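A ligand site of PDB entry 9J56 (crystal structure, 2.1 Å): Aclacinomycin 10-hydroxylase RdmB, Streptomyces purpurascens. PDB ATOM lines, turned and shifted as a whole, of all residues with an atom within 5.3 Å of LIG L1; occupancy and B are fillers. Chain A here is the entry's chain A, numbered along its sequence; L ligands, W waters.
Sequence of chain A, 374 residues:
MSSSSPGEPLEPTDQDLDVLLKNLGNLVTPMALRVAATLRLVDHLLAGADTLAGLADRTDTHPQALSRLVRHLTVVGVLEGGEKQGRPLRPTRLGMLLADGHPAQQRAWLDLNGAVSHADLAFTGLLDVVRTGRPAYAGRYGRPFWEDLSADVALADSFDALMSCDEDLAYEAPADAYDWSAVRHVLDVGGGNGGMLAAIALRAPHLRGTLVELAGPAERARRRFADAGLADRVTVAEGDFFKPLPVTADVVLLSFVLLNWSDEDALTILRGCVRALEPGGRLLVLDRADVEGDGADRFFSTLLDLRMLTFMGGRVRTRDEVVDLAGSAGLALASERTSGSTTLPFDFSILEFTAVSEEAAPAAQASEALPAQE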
ATOM      1  N   TRP A 146     -22.984  -7.903 -23.682  1.00  0.00           N
ATOM      2  CA  TRP A 146     -23.731  -7.882 -24.931  1.00  0.00           C
ATOM      3  C   TRP A 146     -24.506  -9.186 -25.141  1.00  0.00           C
ATOM      4  O   TRP A 146     -25.665  -9.162 -25.563  1.00  0.00           O
ATOM      5  CB  TRP A 146     -22.794  -7.596 -26.112  1.00  0.00           C
ATOM      6  CG  TRP A 146     -22.259  -6.180 -26.053  1.00  0.00           C
ATOM      7  CD1 TRP A 146     -20.973  -5.796 -25.839  1.00  0.00           C
ATOM      8  CD2 TRP A 146     -23.027  -4.972 -26.163  1.00  0.00           C
ATOM      9  NE1 TRP A 146     -20.883  -4.425 -25.811  1.00  0.00           N
ATOM     10  CE2 TRP A 146     -22.124  -3.894 -26.010  1.00  0.00           C
ATOM     11  CE3 TRP A 146     -24.379  -4.693 -26.380  1.00  0.00           C
ATOM     12  CZ2 TRP A 146     -22.541  -2.554 -26.065  1.00  0.00           C
ATOM     13  CZ3 TRP A 146     -24.794  -3.376 -26.428  1.00  0.00           C
ATOM     14  CH2 TRP A 146     -23.880  -2.323 -26.277  1.00  0.00           C
ATOM     15  N   PHE A 159     -31.894  -0.537 -22.218  1.00  0.00           N
ATOM     16  CA  PHE A 159     -30.633   0.088 -22.587  1.00  0.00           C
ATOM     17  C   PHE A 159     -30.809   0.983 -23.804  1.00  0.00           C
ATOM     18  O   PHE A 159     -30.403   2.156 -23.789  1.00  0.00           O
ATOM     19  CB  PHE A 159     -29.562  -0.969 -22.867  1.00  0.00           C
ATOM     20  CG  PHE A 159     -28.299  -0.384 -23.321  1.00  0.00           C
ATOM     21  CD1 PHE A 159     -27.543   0.397 -22.453  1.00  0.00           C
ATOM     22  CD2 PHE A 159     -27.882  -0.521 -24.621  1.00  0.00           C
ATOM     23  CE1 PHE A 159     -26.369   0.970 -22.876  1.00  0.00           C
ATOM     24  CE2 PHE A 159     -26.721   0.071 -25.064  1.00  0.00           C
ATOM     25  CZ  PHE A 159     -25.964   0.812 -24.174  1.00  0.00           C
ATOM     26  N   ASP A 160     -31.421   0.460 -24.868  1.00  0.00           N
ATOM     27  CA  ASP A 160     -31.676   1.278 -26.048  1.00  0.00           C
ATOM     28  C   ASP A 160     -32.484   2.520 -25.698  1.00  0.00           C
ATOM     29  O   ASP A 160     -32.242   3.596 -26.241  1.00  0.00           O
ATOM     30  CB  ASP A 160     -32.416   0.455 -27.106  1.00  0.00           C
ATOM     31  CG  ASP A 160     -31.697  -0.852 -27.432  1.00  0.00           C
ATOM     32  OD1 ASP A 160     -30.443  -0.913 -27.307  1.00  0.00           O
ATOM     33  OD2 ASP A 160     -32.402  -1.824 -27.810  1.00  0.00           O
ATOM     34  N   MET A 163     -30.178   5.201 -24.098  1.00  0.00           N
ATOM     35  CA  MET A 163     -29.267   5.795 -25.069  1.00  0.00           C
ATOM     36  C   MET A 163     -29.988   6.736 -26.041  1.00  0.00           C
ATOM     37  O   MET A 163     -29.392   7.684 -26.569  1.00  0.00           O
ATOM     38  CB  MET A 163     -28.578   4.671 -25.859  1.00  0.00           C
ATOM     39  CG  MET A 163     -27.310   4.038 -25.254  1.00  0.00           C
ATOM     40  SD  MET A 163     -26.152   5.151 -24.401  1.00  0.00           S
ATOM     41  CE  MET A 163     -26.616   4.804 -22.726  1.00  0.00           C
ATOM     42  N   ASP A 188     -24.513   5.245 -40.405  1.00  0.00           N
ATOM     43  CA  ASP A 188     -24.354   5.275 -38.939  1.00  0.00           C
ATOM     44  C   ASP A 188     -24.117   3.853 -38.446  1.00  0.00           C
ATOM     45  O   ASP A 188     -25.028   3.024 -38.442  1.00  0.00           O
ATOM     46  CB  ASP A 188     -25.551   5.877 -38.219  1.00  0.00           C
ATOM     47  CG  ASP A 188     -25.233   6.260 -36.758  1.00  0.00           C
ATOM     48  OD1 ASP A 188     -24.233   5.766 -36.213  1.00  0.00           O
ATOM     49  OD2 ASP A 188     -26.037   6.993 -36.121  1.00  0.00           O
ATOM     50  N   VAL A 189     -22.904   3.600 -37.958  1.00  0.00           N
ATOM     51  CA  VAL A 189     -22.480   2.276 -37.537  1.00  0.00           C
ATOM     52  C   VAL A 189     -22.716   2.161 -36.030  1.00  0.00           C
ATOM     53  O   VAL A 189     -22.107   2.889 -35.241  1.00  0.00           O
ATOM     54  CB  VAL A 189     -21.008   2.047 -37.904  1.00  0.00           C
ATOM     55  CG1 VAL A 189     -20.505   0.713 -37.390  1.00  0.00           C
ATOM     56  CG2 VAL A 189     -20.811   2.167 -39.425  1.00  0.00           C
ATOM     57  N   GLY A 190     -23.600   1.247 -35.634  1.00  0.00           N
ATOM     58  CA  GLY A 190     -24.038   1.181 -34.241  1.00  0.00           C
ATOM     59  C   GLY A 190     -24.808   2.426 -33.805  1.00  0.00           C
ATOM     60  O   GLY A 190     -24.634   2.884 -32.671  1.00  0.00           O
ATOM     61  N   GLY A 191     -25.641   2.974 -34.685  1.00  0.00           N
ATOM     62  CA  GLY A 191     -26.336   4.217 -34.392  1.00  0.00           C
ATOM     63  C   GLY A 191     -27.543   4.108 -33.479  1.00  0.00           C
ATOM     64  O   GLY A 191     -28.384   5.023 -33.456  1.00  0.00           O
ATOM     65  N   GLY A 192     -27.665   3.015 -32.707  1.00  0.00           N
ATOM     66  CA  GLY A 192     -28.763   2.906 -31.758  1.00  0.00           C
ATOM     67  C   GLY A 192     -30.092   2.787 -32.470  1.00  0.00           C
ATOM     68  O   GLY A 192     -30.192   2.155 -33.529  1.00  0.00           O
ATOM     69  N   MET A 196     -29.729  10.011 -33.915  1.00  0.00           N
ATOM     70  CA  MET A 196     -28.713  10.862 -34.535  1.00  0.00           C
ATOM     71  C   MET A 196     -28.902  10.970 -36.049  1.00  0.00           C
ATOM     72  O   MET A 196     -28.783  12.054 -36.626  1.00  0.00           O
ATOM     73  CB  MET A 196     -27.331  10.317 -34.226  1.00  0.00           C
ATOM     74  CG  MET A 196     -26.212  11.310 -34.437  1.00  0.00           C
ATOM     75  SD  MET A 196     -24.727  10.673 -33.592  1.00  0.00           S
ATOM     76  CE  MET A 196     -24.981  11.343 -31.956  1.00  0.00           C
ATOM     77  N   VAL A 212     -26.639   0.650 -39.364  1.00  0.00           N
ATOM     78  CA  VAL A 212     -26.237  -0.729 -39.075  1.00  0.00           C
ATOM     79  C   VAL A 212     -26.286  -0.953 -37.566  1.00  0.00           C
ATOM     80  O   VAL A 212     -25.673  -0.199 -36.800  1.00  0.00           O
ATOM     81  CB  VAL A 212     -24.834  -1.055 -39.630  1.00  0.00           C
ATOM     82  CG1 VAL A 212     -24.515  -2.502 -39.352  1.00  0.00           C
ATOM     83  CG2 VAL A 212     -24.771  -0.779 -41.113  1.00  0.00           C
ATOM     84  N   GLU A 213     -27.016  -1.971 -37.141  1.00  0.00           N
ATOM     85  CA  GLU A 213     -27.224  -2.176 -35.710  1.00  0.00           C
ATOM     86  C   GLU A 213     -27.631  -3.618 -35.462  1.00  0.00           C
ATOM     87  O   GLU A 213     -27.961  -4.372 -36.382  1.00  0.00           O
ATOM     88  CB  GLU A 213     -28.294  -1.240 -35.147  1.00  0.00           C
ATOM     89  CG  GLU A 213     -27.762  -0.075 -34.329  1.00  0.00           C
ATOM     90  CD  GLU A 213     -27.184  -0.484 -32.978  1.00  0.00           C
ATOM     91  OE1 GLU A 213     -27.236  -1.685 -32.635  1.00  0.00           O
ATOM     92  OE2 GLU A 213     -26.656   0.407 -32.270  1.00  0.00           O
ATOM     93  N   LEU A 214     -27.622  -3.986 -34.177  1.00  0.00           N
ATOM     94  CA  LEU A 214     -28.137  -5.258 -33.724  1.00  0.00           C
ATOM     95  C   LEU A 214     -29.653  -5.319 -33.934  1.00  0.00           C
ATOM     96  O   LEU A 214     -30.306  -4.298 -34.193  1.00  0.00           O
ATOM     97  CB  LEU A 214     -27.778  -5.480 -32.248  1.00  0.00           C
ATOM     98  CG  LEU A 214     -26.268  -5.511 -32.000  1.00  0.00           C
ATOM     99  CD1 LEU A 214     -25.924  -5.554 -30.509  1.00  0.00           C
ATOM    100  CD2 LEU A 214     -25.636  -6.704 -32.728  1.00  0.00           C
ATOM    101  N   PRO A 217     -32.162  -2.753 -31.584  1.00  0.00           N
ATOM    102  CA  PRO A 217     -32.132  -1.346 -32.006  1.00  0.00           C
ATOM    103  C   PRO A 217     -32.494  -1.157 -33.466  1.00  0.00           C
ATOM    104  O   PRO A 217     -33.097  -0.131 -33.799  1.00  0.00           O
ATOM    105  CB  PRO A 217     -30.689  -0.904 -31.715  1.00  0.00           C
ATOM    106  CG  PRO A 217     -30.202  -1.886 -30.663  1.00  0.00           C
ATOM    107  CD  PRO A 217     -30.871  -3.187 -31.015  1.00  0.00           C
ATOM    108  N   GLY A 239     -27.055  -5.823 -38.633  1.00  0.00           N
ATOM    109  CA  GLY A 239     -25.724  -6.289 -38.970  1.00  0.00           C
ATOM    110  C   GLY A 239     -24.814  -6.389 -37.766  1.00  0.00           C
ATOM    111  O   GLY A 239     -25.189  -6.056 -36.642  1.00  0.00           O
ATOM    112  N   ASP A 240     -23.610  -6.871 -38.050  1.00  0.00           N
ATOM    113  CA  ASP A 240     -22.519  -7.003 -37.088  1.00  0.00           C
ATOM    114  C   ASP A 240     -21.377  -6.121 -37.560  1.00  0.00           C
ATOM    115  O   ASP A 240     -20.818  -6.350 -38.641  1.00  0.00           O
ATOM    116  CB  ASP A 240     -22.082  -8.469 -36.998  1.00  0.00           C
ATOM    117  CG  ASP A 240     -21.104  -8.726 -35.883  1.00  0.00           C
ATOM    118  OD1 ASP A 240     -20.707  -7.761 -35.202  1.00  0.00           O
ATOM    119  OD2 ASP A 240     -20.747  -9.902 -35.675  1.00  0.00           O
ATOM    120  N   PHE A 241     -21.004  -5.105 -36.767  1.00  0.00           N
ATOM    121  CA  PHE A 241     -19.907  -4.280 -37.266  1.00  0.00           C
ATOM    122  C   PHE A 241     -18.529  -4.899 -37.041  1.00  0.00           C
ATOM    123  O   PHE A 241     -17.507  -4.256 -37.329  1.00  0.00           O
ATOM    124  CB  PHE A 241     -19.987  -2.837 -36.731  1.00  0.00           C
ATOM    125  CG  PHE A 241     -20.023  -2.681 -35.216  1.00  0.00           C
ATOM    126  CD1 PHE A 241     -19.278  -3.491 -34.380  1.00  0.00           C
ATOM    127  CD2 PHE A 241     -20.763  -1.658 -34.645  1.00  0.00           C
ATOM    128  CE1 PHE A 241     -19.302  -3.298 -33.004  1.00  0.00           C
ATOM    129  CE2 PHE A 241     -20.793  -1.464 -33.296  1.00  0.00           C
ATOM    130  CZ  PHE A 241     -20.064  -2.289 -32.465  1.00  0.00           C
ATOM    131  N   PHE A 242     -18.453  -6.135 -36.585  1.00  0.00           N
ATOM    132  CA  PHE A 242     -17.213  -6.886 -36.692  1.00  0.00           C
ATOM    133  C   PHE A 242     -17.103  -7.621 -38.019  1.00  0.00           C
ATOM    134  O   PHE A 242     -16.058  -8.198 -38.309  1.00  0.00           O
ATOM    135  CB  PHE A 242     -17.079  -7.852 -35.517  1.00  0.00           C
ATOM    136  CG  PHE A 242     -16.935  -7.139 -34.208  1.00  0.00           C
ATOM    137  CD1 PHE A 242     -15.775  -6.412 -33.933  1.00  0.00           C
ATOM    138  CD2 PHE A 242     -17.950  -7.147 -33.276  1.00  0.00           C
ATOM    139  CE1 PHE A 242     -15.636  -5.734 -32.731  1.00  0.00           C
ATOM    140  CE2 PHE A 242     -17.826  -6.484 -32.078  1.00  0.00           C
ATOM    141  CZ  PHE A 242     -16.670  -5.774 -31.802  1.00  0.00           C
ATOM    142  N   SER A 255     -20.718   6.802 -33.183  1.00  0.00           N
ATOM    143  CA  SER A 255     -21.106   7.625 -32.035  1.00  0.00           C
ATOM    144  C   SER A 255     -21.082   6.766 -30.761  1.00  0.00           C
ATOM    145  O   SER A 255     -21.925   5.886 -30.590  1.00  0.00           O
ATOM    146  CB  SER A 255     -22.482   8.237 -32.267  1.00  0.00           C
ATOM    147  OG  SER A 255     -22.839   9.064 -31.183  1.00  0.00           O
ATOM    148  N   PHE A 256     -20.155   7.077 -29.861  1.00  0.00           N
ATOM    149  CA  PHE A 256     -20.024   6.375 -28.580  1.00  0.00           C
ATOM    150  C   PHE A 256     -20.107   4.872 -28.773  1.00  0.00           C
ATOM    151  O   PHE A 256     -20.884   4.161 -28.142  1.00  0.00           O
ATOM    152  CB  PHE A 256     -21.054   6.885 -27.566  1.00  0.00           C
ATOM    153  CG  PHE A 256     -20.643   8.197 -26.957  1.00  0.00           C
ATOM    154  CD1 PHE A 256     -20.910   9.399 -27.614  1.00  0.00           C
ATOM    155  CD2 PHE A 256     -19.910   8.228 -25.771  1.00  0.00           C
ATOM    156  CE1 PHE A 256     -20.489  10.612 -27.078  1.00  0.00           C
ATOM    157  CE2 PHE A 256     -19.485   9.434 -25.228  1.00  0.00           C
ATOM    158  CZ  PHE A 256     -19.779  10.624 -25.880  1.00  0.00           C
ATOM    159  N   VAL A 257     -19.292   4.399 -29.704  1.00  0.00           N
ATOM    160  CA  VAL A 257     -19.099   2.978 -29.951  1.00  0.00           C
ATOM    161  C   VAL A 257     -17.731   2.516 -29.461  1.00  0.00           C
ATOM    162  O   VAL A 257     -17.633   1.541 -28.717  1.00  0.00           O
ATOM    163  CB  VAL A 257     -19.295   2.637 -31.435  1.00  0.00           C
ATOM    164  CG1 VAL A 257     -18.643   1.300 -31.776  1.00  0.00           C
ATOM    165  CG2 VAL A 257     -20.765   2.614 -31.777  1.00  0.00           C
ATOM    166  N   ASN A 260     -16.674   1.150 -25.949  1.00  0.00           N
ATOM    167  CA  ASN A 260     -17.166  -0.117 -25.428  1.00  0.00           C
ATOM    168  C   ASN A 260     -16.194  -1.247 -25.638  1.00  0.00           C
ATOM    169  O   ASN A 260     -16.453  -2.364 -25.170  1.00  0.00           O
ATOM    170  CB  ASN A 260     -18.483  -0.529 -26.095  1.00  0.00           C
ATOM    171  CG  ASN A 260     -19.580   0.479 -25.953  1.00  0.00           C
ATOM    172  OD1 ASN A 260     -19.611   1.310 -25.031  1.00  0.00           O
ATOM    173  ND2 ASN A 260     -20.535   0.389 -26.866  1.00  0.00           N
ATOM    174  N   TRP A 261     -15.087  -1.004 -26.339  1.00  0.00           N
ATOM    175  CA  TRP A 261     -14.275  -2.064 -26.916  1.00  0.00           C
ATOM    176  C   TRP A 261     -12.817  -1.925 -26.530  1.00  0.00           C
ATOM    177  O   TRP A 261     -12.320  -0.832 -26.236  1.00  0.00           O
ATOM    178  CB  TRP A 261     -14.409  -2.078 -28.445  1.00  0.00           C
ATOM    179  CG  TRP A 261     -15.811  -2.285 -28.826  1.00  0.00           C
ATOM    180  CD1 TRP A 261     -16.689  -1.345 -29.278  1.00  0.00           C
ATOM    181  CD2 TRP A 261     -16.528  -3.508 -28.716  1.00  0.00           C
ATOM    182  NE1 TRP A 261     -17.917  -1.921 -29.485  1.00  0.00           N
ATOM    183  CE2 TRP A 261     -17.852  -3.255 -29.147  1.00  0.00           C
ATOM    184  CE3 TRP A 261     -16.184  -4.813 -28.316  1.00  0.00           C
ATOM    185  CZ2 TRP A 261     -18.820  -4.246 -29.188  1.00  0.00           C
ATOM    186  CZ3 TRP A 261     -17.156  -5.797 -28.364  1.00  0.00           C
ATOM    187  CH2 TRP A 261     -18.461  -5.513 -28.792  1.00  0.00           C
HETATM  188  N1  LIG L   1     -24.484   5.493 -31.600  1.00  0.00           N
HETATM  189  C1  LIG L   1     -25.291   5.343 -30.402  1.00  0.00           C
HETATM  190  C2  LIG L   1     -24.503   4.552 -29.359  1.00  0.00           C
HETATM  191  C3  LIG L   1     -25.417   3.511 -28.791  1.00  0.00           C
HETATM  192  S1  LIG L   1     -24.355   2.545 -27.682  1.00  0.00           S
HETATM  193  C4  LIG L   1     -25.716   6.687 -29.802  1.00  0.00           C
HETATM  194  O1  LIG L   1     -26.854   6.816 -29.287  1.00  0.00           O
HETATM  195  O2  LIG L   1     -24.911   7.663 -29.823  1.00  0.00           O
HETATM  196  C5  LIG L   1     -23.351   1.350 -28.638  1.00  0.00           C
HETATM  197  C6  LIG L   1     -24.175   0.617 -29.739  1.00  0.00           C
HETATM  198  O3  LIG L   1     -23.435  -0.373 -30.231  1.00  0.00           O
HETATM  199  C7  LIG L   1     -25.486  -0.020 -29.195  1.00  0.00           C
HETATM  200  O4  LIG L   1     -26.595   0.521 -29.779  1.00  0.00           O
HETATM  201  C8  LIG L   1     -25.298  -1.494 -29.598  1.00  0.00           C
HETATM  202  O5  LIG L   1     -26.550  -2.098 -30.110  1.00  0.00           O
HETATM  203  C9  LIG L   1     -24.305  -1.364 -30.751  1.00  0.00           C
HETATM  204  N2  LIG L   1     -23.595  -2.595 -30.997  1.00  0.00           N
HETATM  205  C10 LIG L   1     -22.963  -3.353 -30.098  1.00  0.00           C
HETATM  206  N3  LIG L   1     -22.415  -4.380 -30.748  1.00  0.00           N
HETATM  207  C11 LIG L   1     -22.698  -4.269 -32.042  1.00  0.00           C
HETATM  208  C12 LIG L   1     -22.376  -5.065 -33.120  1.00  0.00           C
HETATM  209  N4  LIG L   1     -21.601  -6.285 -33.119  1.00  0.00           N
HETATM  210  N5  LIG L   1     -22.785  -4.728 -34.343  1.00  0.00           N
HETATM  211  C13 LIG L   1     -23.523  -3.611 -34.515  1.00  0.00           C
HETATM  212  N6  LIG L   1     -23.841  -2.827 -33.452  1.00  0.00           N
HETATM  213  C14 LIG L   1     -23.431  -3.158 -32.207  1.00  0.00           C
HETATM  214  O1  LG2 L   2     -22.999   3.476 -18.135  1.00  0.00           O
HETATM  215  C1  LG2 L   2     -22.925   3.691 -19.253  1.00  0.00           C
HETATM  216  C2  LG2 L   2     -22.852   5.086 -19.776  1.00  0.00           C
HETATM  217  C3  LG2 L   2     -22.774   5.332 -21.082  1.00  0.00           C
HETATM  218  C4  LG2 L   2     -22.718   6.631 -21.579  1.00  0.00           C
HETATM  219  O2  LG2 L   2     -22.655   6.866 -22.932  1.00  0.00           O
HETATM  220  C5  LG2 L   2     -22.761   7.686 -20.693  1.00  0.00           C
HETATM  221  C6  LG2 L   2     -22.684   9.101 -21.260  1.00  0.00           C
HETATM  222  O3  LG2 L   2     -23.866   9.418 -22.014  1.00  0.00           O
HETATM  223  C7  LG2 L   2     -23.596   9.980 -23.246  1.00  0.00           C
HETATM  224  O4  LG2 L   2     -24.563  11.052 -23.604  1.00  0.00           O
HETATM  225  C8  LG2 L   2     -25.871  10.536 -23.962  1.00  0.00           C
HETATM  226  C9  LG2 L   2     -26.659  11.666 -24.535  1.00  0.00           C
HETATM  227  C10 LG2 L   2     -25.881   9.306 -24.907  1.00  0.00           C
HETATM  228  O5  LG2 L   2     -26.770   9.357 -26.065  1.00  0.00           O
HETATM  229  C11 LG2 L   2     -24.541   8.878 -25.398  1.00  0.00           C
HETATM  230  N1  LG2 L   2     -24.244   9.583 -26.723  1.00  0.00           N
HETATM  231  C12 LG2 L   2     -23.475   8.987 -24.384  1.00  0.00           C
HETATM  232  C13 LG2 L   2     -22.330  10.088 -20.175  1.00  0.00           C
HETATM  233  C14 LG2 L   2     -22.922   9.860 -18.809  1.00  0.00           C
HETATM  234  C15 LG2 L   2     -22.273  10.734 -17.749  1.00  0.00           C
HETATM  235  C16 LG2 L   2     -21.049  10.037 -17.178  1.00  0.00           C
HETATM  236  O6  LG2 L   2     -24.268  10.133 -18.897  1.00  0.00           O
HETATM  237  C17 LG2 L   2     -22.849   8.436 -18.241  1.00  0.00           C
HETATM  238  C18 LG2 L   2     -22.821   7.408 -19.368  1.00  0.00           C
HETATM  239  C19 LG2 L   2     -22.872   6.119 -18.880  1.00  0.00           C
HETATM  240  O7  LG2 L   2     -22.947   5.880 -17.539  1.00  0.00           O
HETATM  241  C20 LG2 L   2     -22.749   4.206 -22.057  1.00  0.00           C
HETATM  242  C21 LG2 L   2     -22.820   2.775 -21.555  1.00  0.00           C
HETATM  243  C22 LG2 L   2     -22.796   1.696 -22.422  1.00  0.00           C
HETATM  244  O8  LG2 L   2     -22.711   1.916 -23.758  1.00  0.00           O
HETATM  245  C23 LG2 L   2     -22.967   0.820 -24.551  1.00  0.00           C
HETATM  246  C24 LG2 L   2     -22.853   0.413 -21.954  1.00  0.00           C
HETATM  247  C25 LG2 L   2     -22.946   0.195 -20.595  1.00  0.00           C
HETATM  248  C26 LG2 L   2     -22.954   1.260 -19.738  1.00  0.00           C
HETATM  249  C27 LG2 L   2     -22.902   2.542 -20.234  1.00  0.00           C
HETATM  250  O9  LG2 L   2     -22.682   4.487 -23.167  1.00  0.00           O
HETATM  251  O   HOH W   1     -29.186   5.793 -29.841  1.00  0.00           O
HETATM  252  O   HOH W   2     -25.677   7.389 -33.489  1.00  0.00           O
HETATM  253  O   HOH W   3     -22.785   5.238 -33.974  1.00  0.00           O
HETATM  254  O   HOH W   4     -28.513  -2.846 -27.938  1.00  0.00           O
HETATM  255  O   HOH W   5     -20.611  -0.758 -29.275  1.00  0.00           O
HETATM  256  O   HOH W   6     -28.971   0.886 -28.365  1.00  0.00           O
HETATM  257  O   HOH W   7     -21.915  -6.945 -29.704  1.00  0.00           O
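OE2 of Glu 213 is in hydrogen-bond range of O4 of LIG L1 (2.5 Å). The backbone carbonyl oxygen (O) of Gly 190 sits at hydrogen-bond distance from a nitrogen (N1) of LIG L1 (2.8 Å). A nitrogen (N5) of LIG L1 is in hydrogen-bond range of the backbone NH of Phe 241, at 3.0 Å. An oxygen (O8) of LG2 L2 lies close to the side-chain amide oxygen (OD1) of Asn 260. The side-chain hydroxyl of Ser 255 lies within hydrogen-bond range of an oxygen (O2) of LIG L1 (2.8 Å). A nitrogen (N1) of LIG L1 sits at hydrogen-bond distance from the backbone carbonyl oxygen (O) of Ser 255 (2.8 Å). A nitrogen (N4) of LIG L1 sits at hydrogen-bond distance from the side-chain carboxylate of Asp 240 (2.7 Å). An oxygen (O5) of LG2 L2 lies within hydrogen-bond range of the backbone carbonyl oxygen of Met 163, 3.2 Å away.
The backbone carbonyl oxygen (O) of Glu 213 is in hydrogen-bond range of the backbone NH (N) of Gly 239. O of Val 212 lies within hydrogen-bond range of N of Gly 190 (2.8 Å). The side-chain carboxylate of Glu 213 sits at hydrogen-bond distance from the backbone NH of Gly 192, at 2.8 Å. OD1 of Asp 188 sits close to N of Gly 191, at 3.5 Å. The side-chain sulfur (SD) of Met 196 sits close to the side-chain hydroxyl (OG) of Ser 255 (3.5 Å). The backbone NH (N) of Phe 242 sits close to the side-chain carboxylate (OD1) of Asp 240 (3.1 Å).
Residues that only touch LIG L1: Trp 146 (3.7 Å), Met 163 (3.8 Å), Gly 191 (3.6 Å), Gly 192 (3.8 Å), Leu 214 (3.5 Å), Pro 217 (3.7 Å), Gly 239 (3.6 Å), Phe 242 (3.8 Å), Phe 256 (3.8 Å), Asn 260 (3.5 Å) and Trp 261 (3.9 Å). Of the 23 residues printed, 16 come within 4 Å of LIG L1.
Water W6 lies within hydrogen-bond range of the side-chain carboxylate (OD1) of Asp 160 (2.6 Å) and an oxygen (O4) of LIG L1 (2.8 Å). Water W2 lies within hydrogen-bond range of the side-chain carboxylate of Asp 188, a nitrogen (N1) of LIG L1 and the side-chain sulfur of Met 196. Water W5 lies within hydrogen-bond range of the side-chain amide nitrogen of Asn 260 (2.7 Å), the indole nitrogen of Trp 261 (2.9 Å) and an oxygen (O3) of LIG L1 (3.0 Å). Water W4 lies within hydrogen-bond range of OD1 of Asp 160 and O5 of LIG L1.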
